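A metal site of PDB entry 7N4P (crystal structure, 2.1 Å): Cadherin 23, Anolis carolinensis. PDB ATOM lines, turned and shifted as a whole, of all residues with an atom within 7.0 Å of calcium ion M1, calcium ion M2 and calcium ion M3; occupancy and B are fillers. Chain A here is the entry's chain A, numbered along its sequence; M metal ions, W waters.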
ATOM      1  N   GLU A  20       1.972 -10.839  13.593  1.00  0.00           N
ATOM      2  CA  GLU A  20       3.330 -10.313  13.787  1.00  0.00           C
ATOM      3  C   GLU A  20       3.363  -9.080  14.716  1.00  0.00           C
ATOM      4  O   GLU A  20       4.454  -8.777  15.130  1.00  0.00           O
ATOM      5  CB  GLU A  20       3.962  -9.948  12.448  1.00  0.00           C
ATOM      6  CG  GLU A  20       3.339  -8.751  11.787  1.00  0.00           C
ATOM      7  CD  GLU A  20       4.070  -8.408  10.490  1.00  0.00           C
ATOM      8  OE1 GLU A  20       5.332  -8.497  10.475  1.00  0.00           O
ATOM      9  OE2 GLU A  20       3.366  -8.066   9.500  1.00  0.00           O
ATOM     10  N   LEU A  69       8.034 -10.893  16.568  1.00  0.00           N
ATOM     11  CA  LEU A  69       7.812 -11.585  15.283  1.00  0.00           C
ATOM     12  C   LEU A  69       7.893 -10.561  14.148  1.00  0.00           C
ATOM     13  O   LEU A  69       7.710  -9.362  14.377  1.00  0.00           O
ATOM     14  CB  LEU A  69       6.427 -12.236  15.345  1.00  0.00           C
ATOM     15  CG  LEU A  69       6.260 -13.288  16.438  1.00  0.00           C
ATOM     16  CD1 LEU A  69       4.799 -13.719  16.519  1.00  0.00           C
ATOM     17  CD2 LEU A  69       7.146 -14.469  16.179  1.00  0.00           C
ATOM     18  N   ASP A  70       8.160 -11.039  12.955  1.00  0.00           N
ATOM     19  CA  ASP A  70       8.192 -10.171  11.742  1.00  0.00           C
ATOM     20  C   ASP A  70       7.874 -11.084  10.558  1.00  0.00           C
ATOM     21  O   ASP A  70       8.783 -11.843  10.121  1.00  0.00           O
ATOM     22  CB  ASP A  70       9.535  -9.490  11.568  1.00  0.00           C
ATOM     23  CG  ASP A  70       9.599  -8.679  10.285  1.00  0.00           C
ATOM     24  OD1 ASP A  70       8.552  -8.448   9.635  1.00  0.00           O
ATOM     25  OD2 ASP A  70      10.688  -8.295   9.957  1.00  0.00           O
ATOM     26  N   ARG A  71       6.632 -11.057  10.114  1.00  0.00           N
ATOM     27  CA  ARG A  71       6.240 -11.911   8.987  1.00  0.00           C
ATOM     28  C   ARG A  71       7.168 -11.696   7.797  1.00  0.00           C
ATOM     29  O   ARG A  71       7.287 -12.616   7.057  1.00  0.00           O
ATOM     30  CB  ARG A  71       4.818 -11.626   8.521  1.00  0.00           C
ATOM     31  CG  ARG A  71       4.346 -12.661   7.522  1.00  0.00           C
ATOM     32  CD  ARG A  71       3.327 -12.107   6.560  1.00  0.00           C
ATOM     33  NE  ARG A  71       3.797 -11.019   5.720  1.00  0.00           N
ATOM     34  CZ  ARG A  71       4.069 -11.091   4.412  1.00  0.00           C
ATOM     35  NH1 ARG A  71       4.003 -12.242   3.787  1.00  0.00           N
ATOM     36  NH2 ARG A  71       4.438 -10.016   3.750  1.00  0.00           N
ATOM     37  N   GLU A  72       7.800 -10.523   7.629  1.00  0.00           N
ATOM     38  CA  GLU A  72       8.551 -10.210   6.396  1.00  0.00           C
ATOM     39  C   GLU A  72       9.946 -10.820   6.523  1.00  0.00           C
ATOM     40  O   GLU A  72      10.659 -10.885   5.532  1.00  0.00           O
ATOM     41  CB  GLU A  72       8.675  -8.714   6.122  1.00  0.00           C
ATOM     42  CG  GLU A  72       7.427  -8.140   5.478  1.00  0.00           C
ATOM     43  CD  GLU A  72       6.223  -7.902   6.384  1.00  0.00           C
ATOM     44  OE1 GLU A  72       6.374  -7.508   7.535  1.00  0.00           O
ATOM     45  OE2 GLU A  72       5.104  -8.112   5.892  1.00  0.00           O
ATOM     46  N   THR A  73      10.333 -11.236   7.712  1.00  0.00           N
ATOM     47  CA  THR A  73      11.623 -11.949   7.847  1.00  0.00           C
ATOM     48  C   THR A  73      11.301 -13.431   7.966  1.00  0.00           C
ATOM     49  O   THR A  73      11.938 -14.200   7.310  1.00  0.00           O
ATOM     50  CB  THR A  73      12.395 -11.444   9.067  1.00  0.00           C
ATOM     51  OG1 THR A  73      12.184 -10.038   9.140  1.00  0.00           O
ATOM     52  CG2 THR A  73      13.869 -11.760   8.974  1.00  0.00           C
ATOM     53  N   GLY A  99       1.086 -14.212  11.308  1.00  0.00           N
ATOM     54  CA  GLY A  99       0.103 -13.422  10.536  1.00  0.00           C
ATOM     55  C   GLY A  99       0.654 -12.068  10.113  1.00  0.00           C
ATOM     56  O   GLY A  99       1.357 -11.380  10.958  1.00  0.00           O
ATOM     57  N   ASP A 100       0.350 -11.661   8.875  1.00  0.00           N
ATOM     58  CA  ASP A 100       0.747 -10.316   8.374  1.00  0.00           C
ATOM     59  C   ASP A 100      -0.075  -9.219   9.057  1.00  0.00           C
ATOM     60  O   ASP A 100      -1.310  -9.396   9.159  1.00  0.00           O
ATOM     61  CB  ASP A 100       0.602 -10.191   6.861  1.00  0.00           C
ATOM     62  CG  ASP A 100       1.132  -8.836   6.388  1.00  0.00           C
ATOM     63  OD1 ASP A 100       2.343  -8.581   6.463  1.00  0.00           O
ATOM     64  OD2 ASP A 100       0.301  -8.043   6.012  1.00  0.00           O
ATOM     65  N   VAL A 101       0.563  -8.113   9.462  1.00  0.00           N
ATOM     66  CA  VAL A 101      -0.120  -6.821   9.671  1.00  0.00           C
ATOM     67  C   VAL A 101       0.463  -5.860   8.641  1.00  0.00           C
ATOM     68  O   VAL A 101       1.589  -6.134   8.082  1.00  0.00           O
ATOM     69  CB  VAL A 101       0.088  -6.281  11.104  1.00  0.00           C
ATOM     70  CG1 VAL A 101       1.300  -5.382  11.226  1.00  0.00           C
ATOM     71  CG2 VAL A 101      -1.136  -5.507  11.584  1.00  0.00           C
ATOM     72  N   ASN A 102      -0.269  -4.778   8.355  1.00  0.00           N
ATOM     73  CA  ASN A 102       0.227  -3.707   7.467  1.00  0.00           C
ATOM     74  C   ASN A 102       1.205  -2.859   8.261  1.00  0.00           C
ATOM     75  O   ASN A 102       0.757  -1.905   8.874  1.00  0.00           O
ATOM     76  CB  ASN A 102      -0.880  -2.823   6.893  1.00  0.00           C
ATOM     77  CG  ASN A 102      -0.331  -1.865   5.849  1.00  0.00           C
ATOM     78  OD1 ASN A 102       0.536  -2.230   5.057  1.00  0.00           O
ATOM     79  ND2 ASN A 102      -0.856  -0.664   5.845  1.00  0.00           N
ATOM     80  N   ASP A 103       2.487  -3.176   8.225  1.00  0.00           N
ATOM     81  CA  ASP A 103       3.498  -2.523   9.091  1.00  0.00           C
ATOM     82  C   ASP A 103       4.607  -1.891   8.252  1.00  0.00           C
ATOM     83  O   ASP A 103       5.595  -1.548   8.851  1.00  0.00           O
ATOM     84  CB  ASP A 103       4.007  -3.485  10.183  1.00  0.00           C
ATOM     85  CG  ASP A 103       4.649  -4.801   9.741  1.00  0.00           C
ATOM     86  OD1 ASP A 103       4.450  -5.207   8.604  1.00  0.00           O
ATOM     87  OD2 ASP A 103       5.324  -5.442  10.584  1.00  0.00           O
ATOM     88  N   ASN A 104       4.497  -1.786   6.916  1.00  0.00           N
ATOM     89  CA  ASN A 104       5.549  -1.164   6.049  1.00  0.00           C
ATOM     90  C   ASN A 104       4.856  -0.122   5.163  1.00  0.00           C
ATOM     91  O   ASN A 104       3.859  -0.461   4.550  1.00  0.00           O
ATOM     92  CB  ASN A 104       6.255  -2.172   5.140  1.00  0.00           C
ATOM     93  CG  ASN A 104       7.046  -3.184   5.934  1.00  0.00           C
ATOM     94  OD1 ASN A 104       8.219  -2.973   6.165  1.00  0.00           O
ATOM     95  ND2 ASN A 104       6.377  -4.174   6.512  1.00  0.00           N
ATOM     96  N   ALA A 105       5.339   1.110   5.193  1.00  0.00           N
ATOM     97  CA  ALA A 105       5.033   2.184   4.220  1.00  0.00           C
ATOM     98  C   ALA A 105       5.736   1.841   2.927  1.00  0.00           C
ATOM     99  O   ALA A 105       6.741   1.138   2.928  1.00  0.00           O
ATOM    100  CB  ALA A 105       5.517   3.531   4.724  1.00  0.00           C
ATOM    101  N   PRO A 106       5.183   2.298   1.773  1.00  0.00           N
ATOM    102  CA  PRO A 106       5.850   2.082   0.486  1.00  0.00           C
ATOM    103  C   PRO A 106       7.284   2.639   0.482  1.00  0.00           C
ATOM    104  O   PRO A 106       7.537   3.635   1.171  1.00  0.00           O
ATOM    105  CB  PRO A 106       4.898   2.784  -0.484  1.00  0.00           C
ATOM    106  CG  PRO A 106       3.539   2.702   0.183  1.00  0.00           C
ATOM    107  CD  PRO A 106       3.851   2.929   1.646  1.00  0.00           C
ATOM    108  N   ASP A 134       6.258  -2.384  -1.690  1.00  0.00           N
ATOM    109  CA  ASP A 134       5.615  -2.526  -0.359  1.00  0.00           C
ATOM    110  C   ASP A 134       5.527  -4.013  -0.106  1.00  0.00           C
ATOM    111  O   ASP A 134       4.859  -4.722  -0.873  1.00  0.00           O
ATOM    112  CB  ASP A 134       4.257  -1.824  -0.317  1.00  0.00           C
ATOM    113  CG  ASP A 134       3.670  -1.707   1.076  1.00  0.00           C
ATOM    114  OD1 ASP A 134       3.684  -2.731   1.780  1.00  0.00           O
ATOM    115  OD2 ASP A 134       3.217  -0.569   1.476  1.00  0.00           O
ATOM    116  N   PRO A 135       6.193  -4.514   0.948  1.00  0.00           N
ATOM    117  CA  PRO A 135       6.328  -5.950   1.186  1.00  0.00           C
ATOM    118  C   PRO A 135       5.186  -6.638   1.962  1.00  0.00           C
ATOM    119  O   PRO A 135       5.210  -7.888   2.093  1.00  0.00           O
ATOM    120  CB  PRO A 135       7.609  -5.961   1.998  1.00  0.00           C
ATOM    121  CG  PRO A 135       7.479  -4.733   2.891  1.00  0.00           C
ATOM    122  CD  PRO A 135       6.859  -3.697   1.998  1.00  0.00           C
ATOM    123  N   ASP A 136       4.200  -5.857   2.420  1.00  0.00           N
ATOM    124  CA  ASP A 136       3.036  -6.354   3.208  1.00  0.00           C
ATOM    125  C   ASP A 136       2.144  -7.227   2.308  1.00  0.00           C
ATOM    126  O   ASP A 136       2.197  -7.033   1.140  1.00  0.00           O
ATOM    127  CB  ASP A 136       2.294  -5.188   3.870  1.00  0.00           C
ATOM    128  CG  ASP A 136       3.115  -4.499   4.955  1.00  0.00           C
ATOM    129  OD1 ASP A 136       3.724  -5.228   5.805  1.00  0.00           O
ATOM    130  OD2 ASP A 136       3.187  -3.247   4.901  1.00  0.00           O
ATOM    131  N   GLN A 137       1.376  -8.142   2.921  1.00  0.00           N
ATOM    132  CA  GLN A 137       0.417  -9.050   2.275  1.00  0.00           C
ATOM    133  C   GLN A 137      -0.811  -8.286   1.772  1.00  0.00           C
ATOM    134  O   GLN A 137      -1.168  -7.291   2.384  1.00  0.00           O
ATOM    135  CB  GLN A 137       0.021 -10.113   3.276  1.00  0.00           C
ATOM    136  CG  GLN A 137       0.270 -11.475   2.694  1.00  0.00           C
ATOM    137  CD  GLN A 137       0.009 -12.575   3.696  1.00  0.00           C
ATOM    138  OE1 GLN A 137      -0.706 -12.403   4.672  1.00  0.00           O
ATOM    139  NE2 GLN A 137       0.566 -13.721   3.381  1.00  0.00           N
ATOM    140  N   ALA A 139      -3.894  -6.104   0.149  1.00  0.00           N
ATOM    141  CA  ALA A 139      -4.152  -4.681  -0.145  1.00  0.00           C
ATOM    142  C   ALA A 139      -3.041  -3.794   0.507  1.00  0.00           C
ATOM    143  O   ALA A 139      -2.588  -2.835  -0.148  1.00  0.00           O
ATOM    144  CB  ALA A 139      -5.543  -4.343   0.351  1.00  0.00           C
ATOM    145  N   GLY A 140      -2.587  -4.145   1.724  1.00  0.00           N
ATOM    146  CA  GLY A 140      -1.488  -3.458   2.427  1.00  0.00           C
ATOM    147  C   GLY A 140      -0.166  -3.528   1.661  1.00  0.00           C
ATOM    148  O   GLY A 140       0.747  -2.711   1.954  1.00  0.00           O
ATOM    149  N   GLY A 141      -0.054  -4.439   0.675  1.00  0.00           N
ATOM    150  CA  GLY A 141       1.127  -4.486  -0.190  1.00  0.00           C
ATOM    151  C   GLY A 141       0.953  -3.850  -1.564  1.00  0.00           C
ATOM    152  O   GLY A 141       1.909  -3.954  -2.378  1.00  0.00           O
ATOM    153  N   SER A 142      -0.238  -3.296  -1.839  1.00  0.00           N
ATOM    154  CA  SER A 142      -0.629  -2.667  -3.142  1.00  0.00           C
ATOM    155  C   SER A 142      -0.573  -1.151  -3.014  1.00  0.00           C
ATOM    156  O   SER A 142      -1.175  -0.628  -2.109  1.00  0.00           O
ATOM    157  CB  SER A 142      -2.005  -3.073  -3.627  1.00  0.00           C
ATOM    158  OG  SER A 142      -2.015  -4.441  -3.940  1.00  0.00           O
ATOM    159  N   ASP A 185      -0.352   2.694   0.387  1.00  0.00           N
ATOM    160  CA  ASP A 185      -0.850   1.309   0.294  1.00  0.00           C
ATOM    161  C   ASP A 185      -2.380   1.313   0.431  1.00  0.00           C
ATOM    162  O   ASP A 185      -2.968   2.350   0.803  1.00  0.00           O
ATOM    163  CB  ASP A 185      -0.041   0.375   1.209  1.00  0.00           C
ATOM    164  CG  ASP A 185      -0.293   0.470   2.701  1.00  0.00           C
ATOM    165  OD1 ASP A 185      -1.416   0.811   3.083  1.00  0.00           O
ATOM    166  OD2 ASP A 185       0.618   0.109   3.422  1.00  0.00           O
ATOM    167  N   GLN A 186      -3.004   0.188   0.097  1.00  0.00           N
ATOM    168  CA  GLN A 186      -4.474   0.069  -0.028  1.00  0.00           C
ATOM    169  C   GLN A 186      -5.061  -0.708   1.171  1.00  0.00           C
ATOM    170  O   GLN A 186      -6.123  -1.271   0.991  1.00  0.00           O
ATOM    171  CB  GLN A 186      -4.806  -0.574  -1.376  1.00  0.00           C
ATOM    172  CG  GLN A 186      -4.215   0.186  -2.560  1.00  0.00           C
ATOM    173  CD  GLN A 186      -4.857  -0.285  -3.845  1.00  0.00           C
ATOM    174  OE1 GLN A 186      -4.191  -0.673  -4.799  1.00  0.00           O
ATOM    175  NE2 GLN A 186      -6.180  -0.301  -3.849  1.00  0.00           N
ATOM    176  N   ASP A 187      -4.394  -0.701   2.329  1.00  0.00           N
ATOM    177  CA  ASP A 187      -4.953  -1.239   3.605  1.00  0.00           C
ATOM    178  C   ASP A 187      -6.261  -0.487   3.894  1.00  0.00           C
ATOM    179  O   ASP A 187      -6.242   0.763   3.890  1.00  0.00           O
ATOM    180  CB  ASP A 187      -3.992  -1.079   4.798  1.00  0.00           C
ATOM    181  CG  ASP A 187      -4.438  -1.797   6.074  1.00  0.00           C
ATOM    182  OD1 ASP A 187      -4.220  -3.016   6.135  1.00  0.00           O
ATOM    183  OD2 ASP A 187      -5.035  -1.147   6.971  1.00  0.00           O
ATOM    184  N   LYS A 190      -5.677   1.034   8.159  1.00  0.00           N
ATOM    185  CA  LYS A 190      -4.514   1.945   8.429  1.00  0.00           C
ATOM    186  C   LYS A 190      -3.644   2.092   7.183  1.00  0.00           C
ATOM    187  O   LYS A 190      -2.541   1.562   7.141  1.00  0.00           O
ATOM    188  CB  LYS A 190      -3.698   1.448   9.639  1.00  0.00           C
ATOM    189  CG  LYS A 190      -2.639   0.383   9.323  1.00  0.00           C
ATOM    190  CD  LYS A 190      -1.960  -0.251  10.541  1.00  0.00           C
ATOM    191  CE  LYS A 190      -2.878  -1.024  11.485  1.00  0.00           C
ATOM    192  NZ  LYS A 190      -2.124  -1.656  12.604  1.00  0.00           N
ATOM    193  N   PRO A 191      -4.066   2.809   6.120  1.00  0.00           N
ATOM    194  CA  PRO A 191      -3.253   2.833   4.910  1.00  0.00           C
ATOM    195  C   PRO A 191      -1.965   3.568   5.287  1.00  0.00           C
ATOM    196  O   PRO A 191      -2.085   4.458   6.069  1.00  0.00           O
ATOM    197  CB  PRO A 191      -4.083   3.631   3.918  1.00  0.00           C
ATOM    198  CG  PRO A 191      -4.933   4.514   4.814  1.00  0.00           C
ATOM    199  CD  PRO A 191      -5.248   3.663   6.027  1.00  0.00           C
ATOM    200  N   LEU A 192      -0.789   3.145   4.820  1.00  0.00           N
ATOM    201  CA  LEU A 192       0.473   3.867   5.077  1.00  0.00           C
ATOM    202  C   LEU A 192       0.950   4.497   3.773  1.00  0.00           C
ATOM    203  O   LEU A 192       0.664   3.920   2.701  1.00  0.00           O
ATOM    204  CB  LEU A 192       1.505   2.899   5.645  1.00  0.00           C
ATOM    205  CG  LEU A 192       1.052   2.191   6.928  1.00  0.00           C
ATOM    206  CD1 LEU A 192       2.132   1.265   7.453  1.00  0.00           C
ATOM    207  CD2 LEU A 192       0.634   3.197   7.992  1.00  0.00           C
HETATM  208 CA    CA M   1       3.687  -7.002   7.389  1.00  0.00          CA
HETATM  209 CA    CA M   2       2.172  -1.622   3.511  1.00  0.00          CA
HETATM  210 CA    CA M   3       6.807  -6.938   9.710  1.00  0.00          CA
HETATM  211  O   HOH W   1       8.138  -5.309   8.790  1.00  0.00           O
HETATM  212  O   HOH W   2       7.667  -6.456  11.644  1.00  0.00           O
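The guanidinium group of Arg 71 lies close to the side-chain carboxylate of Asp 100, 2.9 Å away.
The backbone NH (N) of Glu 20 sits at hydrogen-bond distance from the backbone carbonyl oxygen (O) of Gly 99 (2.8 Å).
The backbone carbonyl oxygen (O) of Lys 190 is in hydrogen-bond range of the side-chain amide nitrogen (ND2) of Asn 102, at 3.1 Å.
The side-chain amide nitrogen (ND2) of Asn 104 sits close to the side-chain carboxylate (OD1) of Asp 103 (3.0 Å).
N of Gly 141 sits close to O of Asp 136 (3.5 Å).
The backbone NH (N) of Asp 185 is in hydrogen-bond range of the backbone carbonyl oxygen (O) of Leu 192 (2.8 Å).
The side-chain carboxylate (OE2) of Glu 72 sits close to the guanidinium group (NH2) of Arg 71, at 2.9 Å.
OD2 of Asp 100 is in hydrogen-bond range of N of Gln 137 (3.3 Å).
Within 4 Å of calcium ion M1: Glu 20, Glu 72, Asp 100, Val 101, Asp 103 and Asp 136.
Within 4 Å of calcium ion M2: Asn 102, Asn 104, Asp 134, Asp 136, Gly 140 and Asp 185.
The nearest printed residue that does not touch calcium ion M2 is Ala 105 (4.5 Å).
The nearest printed residue that does not touch calcium ion M3 is Arg 71 (4.1 Å).
Calcium ion M1 is bound by OD1 of Asp 100 (2.3 Å), OD1 of Asp 103 (2.3 Å), OE2 of Glu 72 (2.3 Å), O of Val 101 (2.4 Å), OD1 of Asp 136 (2.4 Å), OE2 of Glu 20 (2.4 Å) and OE1 of Glu 72 (2.7 Å).
Calcium ion M2 is bound by O of Asn 104 (2.3 Å), OD2 of Asp 185 (2.3 Å), OD1 of Asn 102 (2.3 Å), OD2 of Asp 136 (2.4 Å), O of Gly 140 (2.4 Å), OD2 of Asp 134 (2.5 Å) and OD1 of Asp 134 (2.6 Å).
Calcium ion M2 has seven donor atoms within binding distance.
Calcium ion M3 is bound by water W2, the side-chain carboxylate (OE1) of Glu 20, the side-chain carboxylate (OD2) of Asp 103, the side-chain carboxylate (OE1) of Glu 72, water W1 and the side-chain carboxylate (OD1) of Asp 70.
Calcium ion M3 has six donor atoms within binding distance.
Slightly farther from calcium ion M3 lies the side-chain carboxylate (OD1) of Asp 103 (3.1 Å).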
